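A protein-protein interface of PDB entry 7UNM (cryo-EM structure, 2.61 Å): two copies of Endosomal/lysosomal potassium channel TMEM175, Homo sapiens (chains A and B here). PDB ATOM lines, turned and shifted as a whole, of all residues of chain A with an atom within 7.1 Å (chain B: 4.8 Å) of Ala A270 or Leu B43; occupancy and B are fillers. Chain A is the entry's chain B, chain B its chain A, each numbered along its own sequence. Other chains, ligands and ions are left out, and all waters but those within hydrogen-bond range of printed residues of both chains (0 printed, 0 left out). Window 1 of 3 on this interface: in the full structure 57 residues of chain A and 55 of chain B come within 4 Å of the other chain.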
ATOM      1  N   PHE A 264      -4.968 -16.683   2.173  1.00  0.00           N
ATOM      2  CA  PHE A 264      -6.371 -16.346   2.394  1.00  0.00           C
ATOM      3  C   PHE A 264      -7.283 -17.511   2.021  1.00  0.00           C
ATOM      4  O   PHE A 264      -8.206 -17.864   2.772  1.00  0.00           O
ATOM      5  CB  PHE A 264      -6.725 -15.095   1.589  1.00  0.00           C
ATOM      6  CG  PHE A 264      -7.977 -14.410   2.046  1.00  0.00           C
ATOM      7  CD1 PHE A 264      -7.944 -13.514   3.099  1.00  0.00           C
ATOM      8  CD2 PHE A 264      -9.185 -14.656   1.419  1.00  0.00           C
ATOM      9  CE1 PHE A 264      -9.092 -12.881   3.520  1.00  0.00           C
ATOM     10  CE2 PHE A 264     -10.335 -14.026   1.838  1.00  0.00           C
ATOM     11  CZ  PHE A 264     -10.288 -13.137   2.890  1.00  0.00           C
ATOM     12  N   SER A 265      -7.027 -18.132   0.866  1.00  0.00           N
ATOM     13  CA  SER A 265      -7.839 -19.265   0.435  1.00  0.00           C
ATOM     14  C   SER A 265      -7.714 -20.435   1.403  1.00  0.00           C
ATOM     15  O   SER A 265      -8.711 -21.095   1.725  1.00  0.00           O
ATOM     16  CB  SER A 265      -7.428 -19.688  -0.973  1.00  0.00           C
ATOM     17  OG  SER A 265      -7.424 -18.581  -1.853  1.00  0.00           O
ATOM     18  N   ASP A 266      -6.494 -20.717   1.864  1.00  0.00           N
ATOM     19  CA  ASP A 266      -6.297 -21.794   2.825  1.00  0.00           C
ATOM     20  C   ASP A 266      -7.058 -21.520   4.111  1.00  0.00           C
ATOM     21  O   ASP A 266      -7.660 -22.430   4.690  1.00  0.00           O
ATOM     22  CB  ASP A 266      -4.808 -21.977   3.118  1.00  0.00           C
ATOM     23  CG  ASP A 266      -4.067 -22.648   1.981  1.00  0.00           C
ATOM     24  OD1 ASP A 266      -4.702 -23.406   1.221  1.00  0.00           O
ATOM     25  OD2 ASP A 266      -2.846 -22.426   1.850  1.00  0.00           O
ATOM     26  N   GLY A 267      -7.040 -20.271   4.577  1.00  0.00           N
ATOM     27  CA  GLY A 267      -7.805 -19.936   5.765  1.00  0.00           C
ATOM     28  C   GLY A 267      -9.288 -20.192   5.581  1.00  0.00           C
ATOM     29  O   GLY A 267      -9.943 -20.786   6.442  1.00  0.00           O
ATOM     30  N   VAL A 268      -9.836 -19.758   4.445  1.00  0.00           N
ATOM     31  CA  VAL A 268     -11.264 -19.957   4.197  1.00  0.00           C
ATOM     32  C   VAL A 268     -11.599 -21.448   4.171  1.00  0.00           C
ATOM     33  O   VAL A 268     -12.563 -21.902   4.805  1.00  0.00           O
ATOM     34  CB  VAL A 268     -11.682 -19.262   2.888  1.00  0.00           C
ATOM     35  CG1 VAL A 268     -13.120 -19.609   2.534  1.00  0.00           C
ATOM     36  CG2 VAL A 268     -11.510 -17.757   3.007  1.00  0.00           C
ATOM     37  N   TYR A 269     -10.802 -22.230   3.437  1.00  0.00           N
ATOM     38  CA  TYR A 269     -11.075 -23.660   3.316  1.00  0.00           C
ATOM     39  C   TYR A 269     -10.979 -24.358   4.667  1.00  0.00           C
ATOM     40  O   TYR A 269     -11.828 -25.195   5.007  1.00  0.00           O
ATOM     41  CB  TYR A 269     -10.102 -24.294   2.323  1.00  0.00           C
ATOM     42  CG  TYR A 269     -10.499 -24.134   0.873  1.00  0.00           C
ATOM     43  CD1 TYR A 269     -11.590 -24.812   0.352  1.00  0.00           C
ATOM     44  CD2 TYR A 269      -9.777 -23.309   0.021  1.00  0.00           C
ATOM     45  CE1 TYR A 269     -11.952 -24.672  -0.970  1.00  0.00           C
ATOM     46  CE2 TYR A 269     -10.132 -23.163  -1.302  1.00  0.00           C
ATOM     47  CZ  TYR A 269     -11.219 -23.845  -1.791  1.00  0.00           C
ATOM     48  OH  TYR A 269     -11.578 -23.701  -3.110  1.00  0.00           O
ATOM     49  N   ALA A 270      -9.948 -24.032   5.449  1.00  0.00           N
ATOM     50  CA  ALA A 270      -9.785 -24.648   6.758  1.00  0.00           C
ATOM     51  C   ALA A 270     -10.942 -24.294   7.679  1.00  0.00           C
ATOM     52  O   ALA A 270     -11.421 -25.140   8.439  1.00  0.00           O
ATOM     53  CB  ALA A 270      -8.457 -24.219   7.376  1.00  0.00           C
ATOM     54  N   ILE A 271     -11.412 -23.046   7.624  1.00  0.00           N
ATOM     55  CA  ILE A 271     -12.523 -22.651   8.481  1.00  0.00           C
ATOM     56  C   ILE A 271     -13.788 -23.410   8.106  1.00  0.00           C
ATOM     57  O   ILE A 271     -14.558 -23.826   8.977  1.00  0.00           O
ATOM     58  CB  ILE A 271     -12.731 -21.127   8.421  1.00  0.00           C
ATOM     59  CG1 ILE A 271     -11.704 -20.421   9.305  1.00  0.00           C
ATOM     60  CG2 ILE A 271     -14.138 -20.758   8.867  1.00  0.00           C
ATOM     61  CD1 ILE A 271     -11.890 -20.658  10.798  1.00  0.00           C
ATOM     62  N   VAL A 272     -14.040 -23.583   6.807  1.00  0.00           N
ATOM     63  CA  VAL A 272     -15.229 -24.329   6.392  1.00  0.00           C
ATOM     64  C   VAL A 272     -15.138 -25.778   6.869  1.00  0.00           C
ATOM     65  O   VAL A 272     -16.089 -26.334   7.447  1.00  0.00           O
ATOM     66  CB  VAL A 272     -15.406 -24.244   4.865  1.00  0.00           C
ATOM     67  CG1 VAL A 272     -16.496 -25.191   4.399  1.00  0.00           C
ATOM     68  CG2 VAL A 272     -15.720 -22.818   4.453  1.00  0.00           C
ATOM     69  N   ALA A 273     -13.983 -26.407   6.640  1.00  0.00           N
ATOM     70  CA  ALA A 273     -13.804 -27.786   7.073  1.00  0.00           C
ATOM     71  C   ALA A 273     -13.943 -27.916   8.583  1.00  0.00           C
ATOM     72  O   ALA A 273     -14.404 -28.951   9.078  1.00  0.00           O
ATOM     73  CB  ALA A 273     -12.444 -28.306   6.616  1.00  0.00           C
ATOM     74  N   THR A 274     -13.547 -26.885   9.332  1.00  0.00           N
ATOM     75  CA  THR A 274     -13.701 -26.921  10.781  1.00  0.00           C
ATOM     76  C   THR A 274     -15.161 -26.776  11.189  1.00  0.00           C
ATOM     77  O   THR A 274     -15.633 -27.490  12.082  1.00  0.00           O
ATOM     78  CB  THR A 274     -12.858 -25.819  11.419  1.00  0.00           C
ATOM     79  OG1 THR A 274     -11.483 -26.023  11.083  1.00  0.00           O
ATOM     80  CG2 THR A 274     -13.013 -25.836  12.936  1.00  0.00           C
ATOM     81  N   LEU A 275     -15.886 -25.849  10.558  1.00  0.00           N
ATOM     82  CA  LEU A 275     -17.298 -25.679  10.874  1.00  0.00           C
ATOM     83  C   LEU A 275     -18.059 -26.977  10.671  1.00  0.00           C
ATOM     84  O   LEU A 275     -18.989 -27.285  11.429  1.00  0.00           O
ATOM     85  CB  LEU A 275     -17.905 -24.571  10.012  1.00  0.00           C
ATOM     86  CG  LEU A 275     -17.488 -23.141  10.363  1.00  0.00           C
ATOM     87  CD1 LEU A 275     -17.959 -22.175   9.290  1.00  0.00           C
ATOM     88  CD2 LEU A 275     -18.010 -22.729  11.728  1.00  0.00           C
ATOM     89  N   LEU A 276     -17.669 -27.758   9.662  1.00  0.00           N
ATOM     90  CA  LEU A 276     -18.298 -29.063   9.472  1.00  0.00           C
ATOM     91  C   LEU A 276     -18.167 -29.930  10.725  1.00  0.00           C
ATOM     92  O   LEU A 276     -19.159 -30.478  11.228  1.00  0.00           O
ATOM     93  CB  LEU A 276     -17.679 -29.767   8.266  1.00  0.00           C
ATOM     94  CG  LEU A 276     -17.917 -29.093   6.916  1.00  0.00           C
ATOM     95  CD1 LEU A 276     -17.123 -29.799   5.834  1.00  0.00           C
ATOM     96  CD2 LEU A 276     -19.396 -29.073   6.575  1.00  0.00           C
ATOM     97  N   PHE A 317     -16.581 -33.385   4.233  1.00  0.00           N
ATOM     98  CA  PHE A 317     -15.198 -32.935   4.337  1.00  0.00           C
ATOM     99  C   PHE A 317     -14.475 -33.111   3.009  1.00  0.00           C
ATOM    100  O   PHE A 317     -13.867 -32.169   2.486  1.00  0.00           O
ATOM    101  CB  PHE A 317     -14.487 -33.709   5.451  1.00  0.00           C
ATOM    102  CG  PHE A 317     -13.089 -33.232   5.735  1.00  0.00           C
ATOM    103  CD1 PHE A 317     -12.018 -33.693   4.989  1.00  0.00           C
ATOM    104  CD2 PHE A 317     -12.845 -32.335   6.759  1.00  0.00           C
ATOM    105  CE1 PHE A 317     -10.737 -33.259   5.252  1.00  0.00           C
ATOM    106  CE2 PHE A 317     -11.564 -31.900   7.027  1.00  0.00           C
ATOM    107  CZ  PHE A 317     -10.509 -32.362   6.272  1.00  0.00           C
ATOM    108  N   VAL A 320     -15.053 -30.440   0.425  1.00  0.00           N
ATOM    109  CA  VAL A 320     -14.216 -29.266   0.640  1.00  0.00           C
ATOM    110  C   VAL A 320     -12.760 -29.601   0.343  1.00  0.00           C
ATOM    111  O   VAL A 320     -12.088 -28.902  -0.425  1.00  0.00           O
ATOM    112  CB  VAL A 320     -14.392 -28.738   2.075  1.00  0.00           C
ATOM    113  CG1 VAL A 320     -13.566 -27.478   2.287  1.00  0.00           C
ATOM    114  CG2 VAL A 320     -15.859 -28.471   2.371  1.00  0.00           C
ATOM    115  N   TRP A 324     -10.304 -27.596  -2.395  1.00  0.00           N
ATOM    116  CA  TRP A 324      -8.985 -27.042  -2.123  1.00  0.00           C
ATOM    117  C   TRP A 324      -7.930 -27.720  -2.984  1.00  0.00           C
ATOM    118  O   TRP A 324      -7.072 -27.052  -3.572  1.00  0.00           O
ATOM    119  CB  TRP A 324      -8.644 -27.196  -0.640  1.00  0.00           C
ATOM    120  CG  TRP A 324      -7.242 -26.787  -0.310  1.00  0.00           C
ATOM    121  CD1 TRP A 324      -6.809 -25.536   0.017  1.00  0.00           C
ATOM    122  CD2 TRP A 324      -6.085 -27.631  -0.283  1.00  0.00           C
ATOM    123  NE1 TRP A 324      -5.456 -25.548   0.245  1.00  0.00           N
ATOM    124  CE2 TRP A 324      -4.988 -26.822   0.067  1.00  0.00           C
ATOM    125  CE3 TRP A 324      -5.871 -28.991  -0.523  1.00  0.00           C
ATOM    126  CZ2 TRP A 324      -3.698 -27.328   0.186  1.00  0.00           C
ATOM    127  CZ3 TRP A 324      -4.592 -29.490  -0.407  1.00  0.00           C
ATOM    128  CH2 TRP A 324      -3.521 -28.662  -0.056  1.00  0.00           C
ATOM    129  N   PHE B  39      -1.589 -25.499   4.856  1.00  0.00           N
ATOM    130  CA  PHE B  39      -2.991 -25.866   5.013  1.00  0.00           C
ATOM    131  C   PHE B  39      -3.176 -26.837   6.170  1.00  0.00           C
ATOM    132  O   PHE B  39      -4.118 -26.705   6.964  1.00  0.00           O
ATOM    133  CB  PHE B  39      -3.504 -26.472   3.706  1.00  0.00           C
ATOM    134  CG  PHE B  39      -4.945 -26.883   3.748  1.00  0.00           C
ATOM    135  CD1 PHE B  39      -5.941 -25.947   3.951  1.00  0.00           C
ATOM    136  CD2 PHE B  39      -5.304 -28.208   3.575  1.00  0.00           C
ATOM    137  CE1 PHE B  39      -7.264 -26.324   3.988  1.00  0.00           C
ATOM    138  CE2 PHE B  39      -6.625 -28.588   3.610  1.00  0.00           C
ATOM    139  CZ  PHE B  39      -7.607 -27.645   3.817  1.00  0.00           C
ATOM    140  N   SER B  40      -2.285 -27.825   6.281  1.00  0.00           N
ATOM    141  CA  SER B  40      -2.363 -28.766   7.393  1.00  0.00           C
ATOM    142  C   SER B  40      -2.179 -28.056   8.729  1.00  0.00           C
ATOM    143  O   SER B  40      -2.878 -28.357   9.703  1.00  0.00           O
ATOM    144  CB  SER B  40      -1.312 -29.862   7.224  1.00  0.00           C
ATOM    145  OG  SER B  40      -1.367 -30.417   5.923  1.00  0.00           O
ATOM    146  N   ASP B  41      -1.234 -27.115   8.796  1.00  0.00           N
ATOM    147  CA  ASP B  41      -1.013 -26.365  10.027  1.00  0.00           C
ATOM    148  C   ASP B  41      -2.259 -25.589  10.421  1.00  0.00           C
ATOM    149  O   ASP B  41      -2.670 -25.601  11.586  1.00  0.00           O
ATOM    150  CB  ASP B  41       0.169 -25.412   9.856  1.00  0.00           C
ATOM    151  CG  ASP B  41       1.504 -26.113   9.954  1.00  0.00           C
ATOM    152  OD1 ASP B  41       1.597 -27.132  10.668  1.00  0.00           O
ATOM    153  OD2 ASP B  41       2.468 -25.643   9.316  1.00  0.00           O
ATOM    154  N   ALA B  42      -2.872 -24.900   9.459  1.00  0.00           N
ATOM    155  CA  ALA B  42      -4.085 -24.144   9.755  1.00  0.00           C
ATOM    156  C   ALA B  42      -5.187 -25.065  10.262  1.00  0.00           C
ATOM    157  O   ALA B  42      -5.809 -24.803  11.302  1.00  0.00           O
ATOM    158  CB  ALA B  42      -4.545 -23.389   8.508  1.00  0.00           C
ATOM    159  N   LEU B  43      -5.433 -26.162   9.541  1.00  0.00           N
ATOM    160  CA  LEU B  43      -6.471 -27.097   9.955  1.00  0.00           C
ATOM    161  C   LEU B  43      -6.227 -27.590  11.373  1.00  0.00           C
ATOM    162  O   LEU B  43      -7.126 -27.548  12.219  1.00  0.00           O
ATOM    163  CB  LEU B  43      -6.529 -28.283   8.991  1.00  0.00           C
ATOM    164  CG  LEU B  43      -7.428 -28.156   7.762  1.00  0.00           C
ATOM    165  CD1 LEU B  43      -7.130 -29.280   6.792  1.00  0.00           C
ATOM    166  CD2 LEU B  43      -8.894 -28.173   8.164  1.00  0.00           C
ATOM    167  N   LEU B  44      -5.010 -28.058  11.653  1.00  0.00           N
ATOM    168  CA  LEU B  44      -4.737 -28.671  12.946  1.00  0.00           C
ATOM    169  C   LEU B  44      -4.790 -27.648  14.072  1.00  0.00           C
ATOM    170  O   LEU B  44      -5.263 -27.958  15.168  1.00  0.00           O
ATOM    171  CB  LEU B  44      -3.381 -29.378  12.911  1.00  0.00           C
ATOM    172  CG  LEU B  44      -3.317 -30.617  12.013  1.00  0.00           C
ATOM    173  CD1 LEU B  44      -1.952 -31.272  12.078  1.00  0.00           C
ATOM    174  CD2 LEU B  44      -4.395 -31.617  12.396  1.00  0.00           C
ATOM    175  N   SER B  45      -4.315 -26.425  13.830  1.00  0.00           N
ATOM    176  CA  SER B  45      -4.378 -25.399  14.865  1.00  0.00           C
ATOM    177  C   SER B  45      -5.823 -25.065  15.213  1.00  0.00           C
ATOM    178  O   SER B  45      -6.197 -25.010  16.395  1.00  0.00           O
ATOM    179  CB  SER B  45      -3.628 -24.151  14.406  1.00  0.00           C
ATOM    180  OG  SER B  45      -4.144 -23.673  13.179  1.00  0.00           O
ATOM    181  N   ILE B  46      -6.662 -24.854  14.195  1.00  0.00           N
ATOM    182  CA  ILE B  46      -8.067 -24.572  14.475  1.00  0.00           C
ATOM    183  C   ILE B  46      -8.709 -25.751  15.193  1.00  0.00           C
ATOM    184  O   ILE B  46      -9.482 -25.567  16.140  1.00  0.00           O
ATOM    185  CB  ILE B  46      -8.821 -24.207  13.182  1.00  0.00           C
ATOM    186  CG1 ILE B  46      -8.123 -23.042  12.481  1.00  0.00           C
ATOM    187  CG2 ILE B  46     -10.262 -23.814  13.490  1.00  0.00           C
ATOM    188  CD1 ILE B  46      -8.910 -22.452  11.344  1.00  0.00           C
ATOM    189  N   ILE B  47      -8.402 -26.976  14.761  1.00  0.00           N
ATOM    190  CA  ILE B  47      -8.996 -28.158  15.381  1.00  0.00           C
ATOM    191  C   ILE B  47      -8.599 -28.247  16.848  1.00  0.00           C
ATOM    192  O   ILE B  47      -9.422 -28.574  17.709  1.00  0.00           O
ATOM    193  CB  ILE B  47      -8.592 -29.429  14.611  1.00  0.00           C
ATOM    194  CG1 ILE B  47      -9.252 -29.451  13.230  1.00  0.00           C
ATOM    195  CG2 ILE B  47      -8.974 -30.671  15.399  1.00  0.00           C
ATOM    196  CD1 ILE B  47     -10.744 -29.721  13.250  1.00  0.00           C
ATOM    197  N   MET B 117      -5.634 -35.675   7.348  1.00  0.00           N
ATOM    198  CA  MET B 117      -6.229 -34.524   8.018  1.00  0.00           C
ATOM    199  C   MET B 117      -7.674 -34.806   8.405  1.00  0.00           C
ATOM    200  O   MET B 117      -8.124 -34.410   9.483  1.00  0.00           O
ATOM    201  CB  MET B 117      -6.153 -33.294   7.115  1.00  0.00           C
ATOM    202  CG  MET B 117      -4.757 -32.719   6.946  1.00  0.00           C
ATOM    203  SD  MET B 117      -3.994 -32.231   8.503  1.00  0.00           S
ATOM    204  CE  MET B 117      -2.799 -33.544   8.706  1.00  0.00           C
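NE1 of Trp A324 lies within hydrogen-bond range of OD1 of Asp A266, at 2.5 Å. The backbone carbonyl oxygen (O) of Ala A270 is in hydrogen-bond range of the side-chain hydroxyl (OG1) of Thr A274, 2.8 Å away.
Phe B39 touches Asp A266 (CD1 to OD1, 3.9 Å). Tyr A269 touches Phe B39 (CB to CE1, 3.9 Å). Phe B39 touches Ala A270 (CE1 to N, 3.8 Å). Leu B43 touches Ala A270. Ile A271 touches Ile B46. Ala A273 touches Leu B43 (CB to CD2, 3.9 Å). Thr A274 touches Ile B46 (CG2 to CG2, 3.5 Å). Phe B39 touches Trp A324.
Of the printed residues of chain B, Asp A266 touches Phe B39. Of the printed residues of chain B, Tyr A269 touches Phe B39 (3.9 Å). Ala A270 touches two residues of chain B. Of the printed residues of chain B, Thr A274 touches Ile B46. Of the printed residues of chain A, Phe B39 touches Asp A266, Tyr A269, Ala A270 and Trp A324. Leu B43 touches just these residues of chain A: Ala A270 (3.9 Å) and Ala A273 (3.9 Å). Printed residues of chain A within 4 Å of Ile B46: Ile A271 (3.5 Å) and Thr A274 (3.5 Å). Ile B47 touches none of the printed residues of chain A. The nearest residue of chain B that does not touch Ala A270 is Ala B42 (4.2 Å).
Of the 16 printed residues of chain A, 7 touch a printed residue of chain B. Hydrophobic or aromatic side chains of chain A within 4 Å of the printed part of chain B: Tyr A269, Ile A271, Ala A273 and Trp A324. Among the printed residues, no Asp or Glu carboxylate lies within 4 Å of a Lys or Arg side-chain nitrogen of the other chain.
No position is printed for both chains. Of the 8 pairs that touch across the chains among the printed residues, none has its exchanged pair printed and touching as well.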
